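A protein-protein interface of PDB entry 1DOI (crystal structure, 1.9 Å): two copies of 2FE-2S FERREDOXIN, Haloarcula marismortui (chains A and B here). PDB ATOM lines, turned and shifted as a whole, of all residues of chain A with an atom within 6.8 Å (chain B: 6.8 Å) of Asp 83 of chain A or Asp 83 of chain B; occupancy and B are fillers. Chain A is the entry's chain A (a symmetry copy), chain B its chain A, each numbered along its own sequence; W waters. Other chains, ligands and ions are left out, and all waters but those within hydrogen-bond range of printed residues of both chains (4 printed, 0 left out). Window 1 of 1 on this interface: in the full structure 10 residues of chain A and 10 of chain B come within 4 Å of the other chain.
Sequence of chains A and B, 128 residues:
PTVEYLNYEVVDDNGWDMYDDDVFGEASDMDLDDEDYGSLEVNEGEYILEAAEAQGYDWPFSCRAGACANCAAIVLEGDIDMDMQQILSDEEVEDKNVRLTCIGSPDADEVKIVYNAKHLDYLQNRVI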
ATOM      1  N   TYR A  47      21.385 -14.381   7.426  1.00  0.00           N
ATOM      2  CA  TYR A  47      20.296 -14.749   6.540  1.00  0.00           C
ATOM      3  C   TYR A  47      20.794 -14.965   5.137  1.00  0.00           C
ATOM      4  O   TYR A  47      21.534 -14.109   4.629  1.00  0.00           O
ATOM      5  CB  TYR A  47      19.224 -13.652   6.489  1.00  0.00           C
ATOM      6  CG  TYR A  47      18.514 -13.443   7.820  1.00  0.00           C
ATOM      7  CD1 TYR A  47      17.947 -14.517   8.485  1.00  0.00           C
ATOM      8  CD2 TYR A  47      18.362 -12.161   8.337  1.00  0.00           C
ATOM      9  CE1 TYR A  47      17.207 -14.320   9.664  1.00  0.00           C
ATOM     10  CE2 TYR A  47      17.638 -11.952   9.501  1.00  0.00           C
ATOM     11  CZ  TYR A  47      17.061 -13.025  10.159  1.00  0.00           C
ATOM     12  OH  TYR A  47      16.354 -12.832  11.327  1.00  0.00           O
ATOM     13  N   GLY A  66       8.642 -14.116   7.370  1.00  0.00           N
ATOM     14  CA  GLY A  66       8.205 -15.479   7.566  1.00  0.00           C
ATOM     15  C   GLY A  66       6.707 -15.551   7.510  1.00  0.00           C
ATOM     16  O   GLY A  66       6.105 -16.373   8.234  1.00  0.00           O
ATOM     17  N   ASP A  81      18.400 -23.207   9.123  1.00  0.00           N
ATOM     18  CA  ASP A  81      17.763 -22.997  10.401  1.00  0.00           C
ATOM     19  C   ASP A  81      16.942 -21.761  10.164  1.00  0.00           C
ATOM     20  O   ASP A  81      17.570 -20.758   9.732  1.00  0.00           O
ATOM     21  CB  ASP A  81      18.800 -22.690  11.443  1.00  0.00           C
ATOM     22  CG  ASP A  81      18.288 -22.465  12.849  1.00  0.00           C
ATOM     23  OD1 ASP A  81      17.112 -22.687  13.147  1.00  0.00           O
ATOM     24  OD2 ASP A  81      19.121 -22.050  13.647  1.00  0.00           O
ATOM     25  N   MET A  82      15.637 -21.795  10.510  1.00  0.00           N
ATOM     26  CA  MET A  82      14.774 -20.624  10.291  1.00  0.00           C
ATOM     27  C   MET A  82      14.311 -19.954  11.562  1.00  0.00           C
ATOM     28  O   MET A  82      14.399 -20.514  12.623  1.00  0.00           O
ATOM     29  CB  MET A  82      13.463 -20.933   9.522  1.00  0.00           C
ATOM     30  CG  MET A  82      13.632 -21.380   8.115  1.00  0.00           C
ATOM     31  SD  MET A  82      12.010 -21.698   7.433  1.00  0.00           S
ATOM     32  CE  MET A  82      11.605 -23.300   8.083  1.00  0.00           C
ATOM     33  N   ASP A  83      13.924 -18.687  11.534  1.00  0.00           N
ATOM     34  CA  ASP A  83      13.236 -18.089  12.658  1.00  0.00           C
ATOM     35  C   ASP A  83      11.842 -18.675  12.759  1.00  0.00           C
ATOM     36  O   ASP A  83      11.417 -19.377  11.854  1.00  0.00           O
ATOM     37  CB  ASP A  83      13.104 -16.562  12.514  1.00  0.00           C
ATOM     38  CG  ASP A  83      14.401 -15.767  12.620  1.00  0.00           C
ATOM     39  OD1 ASP A  83      15.341 -16.155  13.303  1.00  0.00           O
ATOM     40  OD2 ASP A  83      14.446 -14.718  11.995  1.00  0.00           O
ATOM     41  N   MET A  84      11.080 -18.404  13.831  1.00  0.00           N
ATOM     42  CA  MET A  84       9.751 -18.995  13.971  1.00  0.00           C
ATOM     43  C   MET A  84       8.886 -18.534  12.820  1.00  0.00           C
ATOM     44  O   MET A  84       8.997 -17.379  12.401  1.00  0.00           O
ATOM     45  CB  MET A  84       8.982 -18.562  15.188  1.00  0.00           C
ATOM     46  CG  MET A  84       9.690 -18.667  16.482  1.00  0.00           C
ATOM     47  SD  MET A  84       8.781 -17.796  17.814  1.00  0.00           S
ATOM     48  CE  MET A  84       8.061 -16.443  16.927  1.00  0.00           C
ATOM     49  N   GLN A  85       8.042 -19.426  12.325  1.00  0.00           N
ATOM     50  CA  GLN A  85       7.194 -19.099  11.186  1.00  0.00           C
ATOM     51  C   GLN A  85       6.019 -20.043  11.313  1.00  0.00           C
ATOM     52  O   GLN A  85       6.159 -21.159  11.831  1.00  0.00           O
ATOM     53  CB  GLN A  85       7.998 -19.300   9.882  1.00  0.00           C
ATOM     54  CG  GLN A  85       8.637 -20.676   9.553  1.00  0.00           C
ATOM     55  CD  GLN A  85       7.604 -21.688   9.104  1.00  0.00           C
ATOM     56  OE1 GLN A  85       6.495 -21.358   8.646  1.00  0.00           O
ATOM     57  NE2 GLN A  85       7.912 -22.967   9.276  1.00  0.00           N
ATOM     58  N   GLN A  86       4.844 -19.605  10.918  1.00  0.00           N
ATOM     59  CA  GLN A  86       3.653 -20.414  11.021  1.00  0.00           C
ATOM     60  C   GLN A  86       3.126 -20.624   9.604  1.00  0.00           C
ATOM     61  O   GLN A  86       2.088 -21.246   9.409  1.00  0.00           O
ATOM     62  CB  GLN A  86       2.584 -19.688  11.888  1.00  0.00           C
ATOM     63  CG  GLN A  86       2.935 -19.502  13.364  1.00  0.00           C
ATOM     64  CD  GLN A  86       3.890 -18.341  13.590  1.00  0.00           C
ATOM     65  OE1 GLN A  86       4.928 -18.417  14.264  1.00  0.00           O
ATOM     66  NE2 GLN A  86       3.604 -17.183  13.002  1.00  0.00           N
ATOM     67  N   LEU A 100      12.546 -20.712   4.263  1.00  0.00           N
ATOM     68  CA  LEU A 100      12.254 -19.339   3.793  1.00  0.00           C
ATOM     69  C   LEU A 100      13.585 -18.618   3.852  1.00  0.00           C
ATOM     70  O   LEU A 100      14.178 -18.505   4.927  1.00  0.00           O
ATOM     71  CB  LEU A 100      11.208 -18.730   4.691  1.00  0.00           C
ATOM     72  CG  LEU A 100       9.839 -19.475   4.569  1.00  0.00           C
ATOM     73  CD1 LEU A 100       8.895 -19.082   5.673  1.00  0.00           C
ATOM     74  CD2 LEU A 100       9.216 -19.164   3.193  1.00  0.00           C
ATOM     75  N   CYS A 102      14.424 -15.509   3.653  1.00  0.00           N
ATOM     76  CA  CYS A 102      14.553 -14.216   4.327  1.00  0.00           C
ATOM     77  C   CYS A 102      14.835 -14.373   5.814  1.00  0.00           C
ATOM     78  O   CYS A 102      15.289 -13.479   6.513  1.00  0.00           O
ATOM     79  CB  CYS A 102      13.267 -13.330   4.179  1.00  0.00           C
ATOM     80  SG  CYS A 102      11.739 -13.972   4.975  1.00  0.00           S
ATOM     81  N   ILE A 103      14.437 -15.494   6.367  1.00  0.00           N
ATOM     82  CA  ILE A 103      14.607 -15.697   7.794  1.00  0.00           C
ATOM     83  C   ILE A 103      15.390 -16.962   8.088  1.00  0.00           C
ATOM     84  O   ILE A 103      15.294 -17.480   9.175  1.00  0.00           O
ATOM     85  CB  ILE A 103      13.201 -15.764   8.586  1.00  0.00           C
ATOM     86  CG1 ILE A 103      12.300 -16.824   8.073  1.00  0.00           C
ATOM     87  CG2 ILE A 103      12.550 -14.377   8.560  1.00  0.00           C
ATOM     88  CD1 ILE A 103      11.103 -16.982   9.000  1.00  0.00           C
ATOM     89  N   GLY A 104      16.198 -17.477   7.213  1.00  0.00           N
ATOM     90  CA  GLY A 104      16.904 -18.688   7.452  1.00  0.00           C
ATOM     91  C   GLY A 104      18.368 -18.478   7.164  1.00  0.00           C
ATOM     92  O   GLY A 104      18.787 -17.715   6.294  1.00  0.00           O
ATOM     93  N   SER A 105      19.178 -19.153   7.963  1.00  0.00           N
ATOM     94  CA  SER A 105      20.614 -19.145   7.811  1.00  0.00           C
ATOM     95  C   SER A 105      21.078 -20.601   7.574  1.00  0.00           C
ATOM     96  O   SER A 105      20.328 -21.523   7.883  1.00  0.00           O
ATOM     97  CB  SER A 105      21.186 -18.512   9.107  1.00  0.00           C
ATOM     98  OG  SER A 105      20.858 -19.187  10.313  1.00  0.00           O
ATOM     99  N   TYR B  47       6.109 -15.926  22.148  1.00  0.00           N
ATOM    100  CA  TYR B  47       7.180 -16.542  22.911  1.00  0.00           C
ATOM    101  C   TYR B  47       6.667 -17.077  24.221  1.00  0.00           C
ATOM    102  O   TYR B  47       5.958 -16.345  24.926  1.00  0.00           O
ATOM    103  CB  TYR B  47       8.291 -15.532  23.225  1.00  0.00           C
ATOM    104  CG  TYR B  47       9.015 -15.029  21.983  1.00  0.00           C
ATOM    105  CD1 TYR B  47       9.545 -15.928  21.072  1.00  0.00           C
ATOM    106  CD2 TYR B  47       9.218 -13.666  21.796  1.00  0.00           C
ATOM    107  CE1 TYR B  47      10.297 -15.475  19.974  1.00  0.00           C
ATOM    108  CE2 TYR B  47       9.955 -13.205  20.717  1.00  0.00           C
ATOM    109  CZ  TYR B  47      10.494 -14.104  19.812  1.00  0.00           C
ATOM    110  OH  TYR B  47      11.214 -13.657  18.723  1.00  0.00           O
ATOM    111  N   GLY B  66      18.853 -16.166  22.207  1.00  0.00           N
ATOM    112  CA  GLY B  66      19.238 -17.454  21.680  1.00  0.00           C
ATOM    113  C   GLY B  66      20.733 -17.594  21.709  1.00  0.00           C
ATOM    114  O   GLY B  66      21.306 -18.235  20.803  1.00  0.00           O
ATOM    115  N   ASP B  81       8.766 -24.171  18.319  1.00  0.00           N
ATOM    116  CA  ASP B  81       9.417 -23.677  17.128  1.00  0.00           C
ATOM    117  C   ASP B  81      10.283 -22.569  17.658  1.00  0.00           C
ATOM    118  O   ASP B  81       9.691 -21.681  18.326  1.00  0.00           O
ATOM    119  CB  ASP B  81       8.397 -23.084  16.199  1.00  0.00           C
ATOM    120  CG  ASP B  81       8.923 -22.540  14.889  1.00  0.00           C
ATOM    121  OD1 ASP B  81      10.092 -22.726  14.540  1.00  0.00           O
ATOM    122  OD2 ASP B  81       8.111 -21.911  14.222  1.00  0.00           O
ATOM    123  N   MET B  82      11.588 -22.567  17.308  1.00  0.00           N
ATOM    124  CA  MET B  82      12.493 -21.519  17.804  1.00  0.00           C
ATOM    125  C   MET B  82      12.987 -20.574  16.735  1.00  0.00           C
ATOM    126  O   MET B  82      12.883 -20.853  15.569  1.00  0.00           O
ATOM    127  CB  MET B  82      13.788 -22.056  18.468  1.00  0.00           C
ATOM    128  CG  MET B  82      13.595 -22.829  19.723  1.00  0.00           C
ATOM    129  SD  MET B  82      15.201 -23.366  20.298  1.00  0.00           S
ATOM    130  CE  MET B  82      15.547 -24.774  19.272  1.00  0.00           C
ATOM    131  N   ASP B  83      13.422 -19.369  17.072  1.00  0.00           N
ATOM    132  CA  ASP B  83      14.136 -18.540  16.126  1.00  0.00           C
ATOM    133  C   ASP B  83      15.508 -19.135  15.878  1.00  0.00           C
ATOM    134  O   ASP B  83      15.902 -20.054  16.580  1.00  0.00           O
ATOM    135  CB  ASP B  83      14.326 -17.101  16.641  1.00  0.00           C
ATOM    136  CG  ASP B  83      13.061 -16.256  16.740  1.00  0.00           C
ATOM    137  OD1 ASP B  83      12.109 -16.428  15.986  1.00  0.00           O
ATOM    138  OD2 ASP B  83      13.052 -15.391  17.604  1.00  0.00           O
ATOM    139  N   MET B  84      16.284 -18.638  14.901  1.00  0.00           N
ATOM    140  CA  MET B  84      17.592 -19.226  14.615  1.00  0.00           C
ATOM    141  C   MET B  84      18.468 -19.095  15.839  1.00  0.00           C
ATOM    142  O   MET B  84      18.398 -18.076  16.530  1.00  0.00           O
ATOM    143  CB  MET B  84      18.382 -18.536  13.538  1.00  0.00           C
ATOM    144  CG  MET B  84      17.676 -18.293  12.261  1.00  0.00           C
ATOM    145  SD  MET B  84      18.624 -17.156  11.179  1.00  0.00           S
ATOM    146  CE  MET B  84      19.391 -16.091  12.368  1.00  0.00           C
ATOM    147  N   GLN B  85      19.275 -20.112  16.096  1.00  0.00           N
ATOM    148  CA  GLN B  85      20.129 -20.108  17.277  1.00  0.00           C
ATOM    149  C   GLN B  85      21.268 -21.035  16.915  1.00  0.00           C
ATOM    150  O   GLN B  85      21.088 -21.984  16.139  1.00  0.00           O
ATOM    151  CB  GLN B  85      19.311 -20.593  18.494  1.00  0.00           C
ATOM    152  CG  GLN B  85      18.620 -21.983  18.478  1.00  0.00           C
ATOM    153  CD  GLN B  85      19.611 -23.112  18.659  1.00  0.00           C
ATOM    154  OE1 GLN B  85      20.730 -22.948  19.179  1.00  0.00           O
ATOM    155  NE2 GLN B  85      19.257 -24.297  18.179  1.00  0.00           N
ATOM    156  N   GLN B  86      22.458 -20.753  17.401  1.00  0.00           N
ATOM    157  CA  GLN B  86      23.617 -21.557  17.096  1.00  0.00           C
ATOM    158  C   GLN B  86      24.129 -22.128  18.416  1.00  0.00           C
ATOM    159  O   GLN B  86      25.142 -22.818  18.446  1.00  0.00           O
ATOM    160  CB  GLN B  86      24.717 -20.680  16.429  1.00  0.00           C
ATOM    161  CG  GLN B  86      24.380 -20.124  15.045  1.00  0.00           C
ATOM    162  CD  GLN B  86      23.471 -18.908  15.117  1.00  0.00           C
ATOM    163  OE1 GLN B  86      22.434 -18.776  14.450  1.00  0.00           O
ATOM    164  NE2 GLN B  86      23.797 -17.942  15.970  1.00  0.00           N
ATOM    165  N   LEU B 100      14.687 -23.170  23.615  1.00  0.00           N
ATOM    166  CA  LEU B 100      15.029 -21.967  24.407  1.00  0.00           C
ATOM    167  C   LEU B 100      13.726 -21.204  24.534  1.00  0.00           C
ATOM    168  O   LEU B 100      13.143 -20.807  23.522  1.00  0.00           O
ATOM    169  CB  LEU B 100      16.102 -21.197  23.681  1.00  0.00           C
ATOM    170  CG  LEU B 100      17.440 -22.000  23.610  1.00  0.00           C
ATOM    171  CD1 LEU B 100      18.404 -21.383  22.632  1.00  0.00           C
ATOM    172  CD2 LEU B 100      18.068 -22.060  25.017  1.00  0.00           C
ATOM    173  N   CYS B 102      13.005 -18.210  25.494  1.00  0.00           N
ATOM    174  CA  CYS B 102      12.928 -16.788  25.160  1.00  0.00           C
ATOM    175  C   CYS B 102      12.648 -16.563  23.681  1.00  0.00           C
ATOM    176  O   CYS B 102      12.231 -15.507  23.226  1.00  0.00           O
ATOM    177  CB  CYS B 102      14.246 -16.014  25.516  1.00  0.00           C
ATOM    178  SG  CYS B 102      15.752 -16.498  24.579  1.00  0.00           S
ATOM    179  N   ILE B 103      13.005 -17.528  22.868  1.00  0.00           N
ATOM    180  CA  ILE B 103      12.834 -17.367  21.436  1.00  0.00           C
ATOM    181  C   ILE B 103      12.005 -18.490  20.843  1.00  0.00           C
ATOM    182  O   ILE B 103      12.087 -18.728  19.662  1.00  0.00           O
ATOM    183  CB  ILE B 103      14.241 -17.290  20.644  1.00  0.00           C
ATOM    184  CG1 ILE B 103      15.098 -18.477  20.877  1.00  0.00           C
ATOM    185  CG2 ILE B 103      14.943 -15.978  21.008  1.00  0.00           C
ATOM    186  CD1 ILE B 103      16.293 -18.447  19.934  1.00  0.00           C
ATOM    187  N   GLY B 104      11.174 -19.174  21.568  1.00  0.00           N
ATOM    188  CA  GLY B 104      10.424 -20.261  21.043  1.00  0.00           C
ATOM    189  C   GLY B 104       8.968 -20.074  21.380  1.00  0.00           C
ATOM    190  O   GLY B 104       8.574 -19.532  22.413  1.00  0.00           O
ATOM    191  N   SER B 105       8.137 -20.500  20.443  1.00  0.00           N
ATOM    192  CA  SER B 105       6.701 -20.475  20.599  1.00  0.00           C
ATOM    193  C   SER B 105       6.181 -21.926  20.474  1.00  0.00           C
ATOM    194  O   SER B 105       6.898 -22.771  19.944  1.00  0.00           O
ATOM    195  CB  SER B 105       6.159 -19.522  19.502  1.00  0.00           C
ATOM    196  OG  SER B 105       6.468 -19.891  18.165  1.00  0.00           O
HETATM  197  O   HOH W   1      21.192 -20.676  12.891  1.00  0.00           O
HETATM  198  O   HOH W   2      16.107 -22.713  15.528  1.00  0.00           O
HETATM  199  O   HOH W   3      11.107 -22.204  12.221  1.00  0.00           O
HETATM  200  O   HOH W   4       6.090 -20.687  15.302  1.00  0.00           O
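The backbone NH (N) of Met 84 of chain B sits at hydrogen-bond distance from the side-chain carboxylate (OD1) of Asp 83 of chain A. OD1 of Asp 83 of chain B lies within hydrogen-bond range of N of Met 84 of chain A (3.1 Å). The backbone NH of Gln 85 of chain A sits at hydrogen-bond distance from the side-chain carboxylate of Asp 81 of chain B. OG of Ser 105 of chain B lies within hydrogen-bond range of SD of Met 84 of chain A. The backbone NH (N) of Gln 85 of chain B sits at hydrogen-bond distance from the side-chain carboxylate (OD2) of Asp 81 of chain A (3.1 Å). O of Met 82 of chain A sits close to O of Met 82 of chain B, at 3.3 Å. The side-chain sulfur of Met 84 of chain B lies within hydrogen-bond range of the side-chain hydroxyl of Ser 105 of chain A (3.1 Å).
O of Ile 103 of chain B is in hydrogen-bond range of N of Asp 83 of chain B (3.0 Å). OD2 of Asp 83 of chain B lies within hydrogen-bond range of OH of Tyr 47 of chain B (2.8 Å). The backbone NH of Asp 81 of chain A is in hydrogen-bond range of the backbone carbonyl oxygen of Ser 105 of chain A (2.8 Å). The backbone NH (N) of Asp 81 of chain B lies within hydrogen-bond range of the backbone carbonyl oxygen (O) of Ser 105 of chain B (2.8 Å). N of Leu 100 of chain B is in hydrogen-bond range of SD of Met 82 of chain B (3.4 Å). OD2 of Asp 83 of chain A lies within hydrogen-bond range of OH of Tyr 47 of chain A (2.8 Å).
Met 84 of chain B touches Tyr 47 of chain A (SD to CE1, 3.5 Å). CA of Met 84 of chain B touches OD2 of Asp 81 of chain A, at 3.4 Å. Met 82 of chain A touches Asp 83 of chain B. Met 82 of chain A touches Met 84 of chain B (O to N, 3.5 Å). C of Asp 83 of chain A touches O of Met 82 of chain B, at 3.7 Å. CA of Asp 83 of chain A touches CA of Asp 83 of chain B, at 3.6 Å. CE1 of Tyr 47 of chain B touches SD of Met 84 of chain A, at 3.5 Å. Met 84 of chain A touches Asp 81 of chain B (CA to OD2, 3.4 Å). Met 84 of chain A touches Met 82 of chain B (N to O, 3.5 Å). Ile 103 of chain A touches Met 84 of chain B.
Asp 83 of chain A touches just these residues of chain B: Met 82 (3.7 Å), Asp 83 (3.6 Å) and Met 84 (3.1 Å). Asp 83 of chain B touches three residues of chain A. Of the printed residues of chain B, Met 84 of chain A touches Tyr 47 (3.5 Å), Asp 81 (3.4 Å), Met 82 (3.5 Å), Asp 83 (3.1 Å), Ile 103 (3.9 Å) and Ser 105 (3.1 Å). Printed residues of chain A within 4 Å of Met 84 of chain B: Tyr 47, Asp 81, Met 82, Asp 83, Ile 103 and Ser 105. Of the printed residues of chain B, Ser 105 of chain A touches Met 84 (3.1 Å). Leu 100 of chain B touches none of the printed residues of chain A.
Of the 13 printed residues of chain A, 8 touch a printed residue of chain B. Printed residues of chain A that touch a printed residue of chain B: Tyr 47, Asp 81, Met 82, Asp 83, Met 84, Gln 85, Ile 103 and Ser 105. Hydrophobic or aromatic side chains of chain A within 4 Å of the printed part of chain B: Tyr 47 and Met 84. Of the 13 printed residues of chain B, 8 touch a printed residue of chain A. Along chain B the printed residues that touch a printed residue of chain A span positions 47 to 105. Among the printed residues, no Asp or Glu carboxylate lies within 4 Å of a Lys or Arg side-chain nitrogen of the other chain.
Tyr 47 of chain A touches Met 84 of chain B, and with the chains exchanged Met 84 of chain A touches Tyr 47 of chain B. Asp 81 of chain A touches Gln 85 of chain B, and with the chains exchanged Gln 85 of chain A touches Asp 81 of chain B. Met 82 of chain A touches Met 84 of chain B, and with the chains exchanged Met 84 of chain A touches Met 82 of chain B. Met 84 of chain A touches Ser 105 of chain B, and with the chains exchanged Ser 105 of chain A touches Met 84 of chain B. Positions printed for both chains: 47, 66, 81, 82, 83, 84, 85, 86, 100, 102, 103, 104 and 105. Of the 18 pairs that touch across the chains among the printed residues, 18 have their exchanged pair printed and touching as well.
Water W3 lies within hydrogen-bond range of OD1 of Asp 81 of chain B (2.6 Å) and O of Asp 83 of chain A (2.9 Å). Water W2 lies within hydrogen-bond range of OD1 of Asp 81 of chain A and O of Asp 83 of chain B. Water W4 lies within hydrogen-bond range of OD2 of Asp 81 of chain B (2.6 Å), OE1 of Gln 86 of chain A (2.8 Å) and OG of Ser 105 of chain B (3.0 Å). Water W1 lies within hydrogen-bond range of the side-chain carboxylate (OD2) of Asp 81 of chain A (2.6 Å), the side-chain amide oxygen (OE1) of Gln 86 of chain B (2.8 Å) and the side-chain hydroxyl (OG) of Ser 105 of chain A (3.0 Å).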
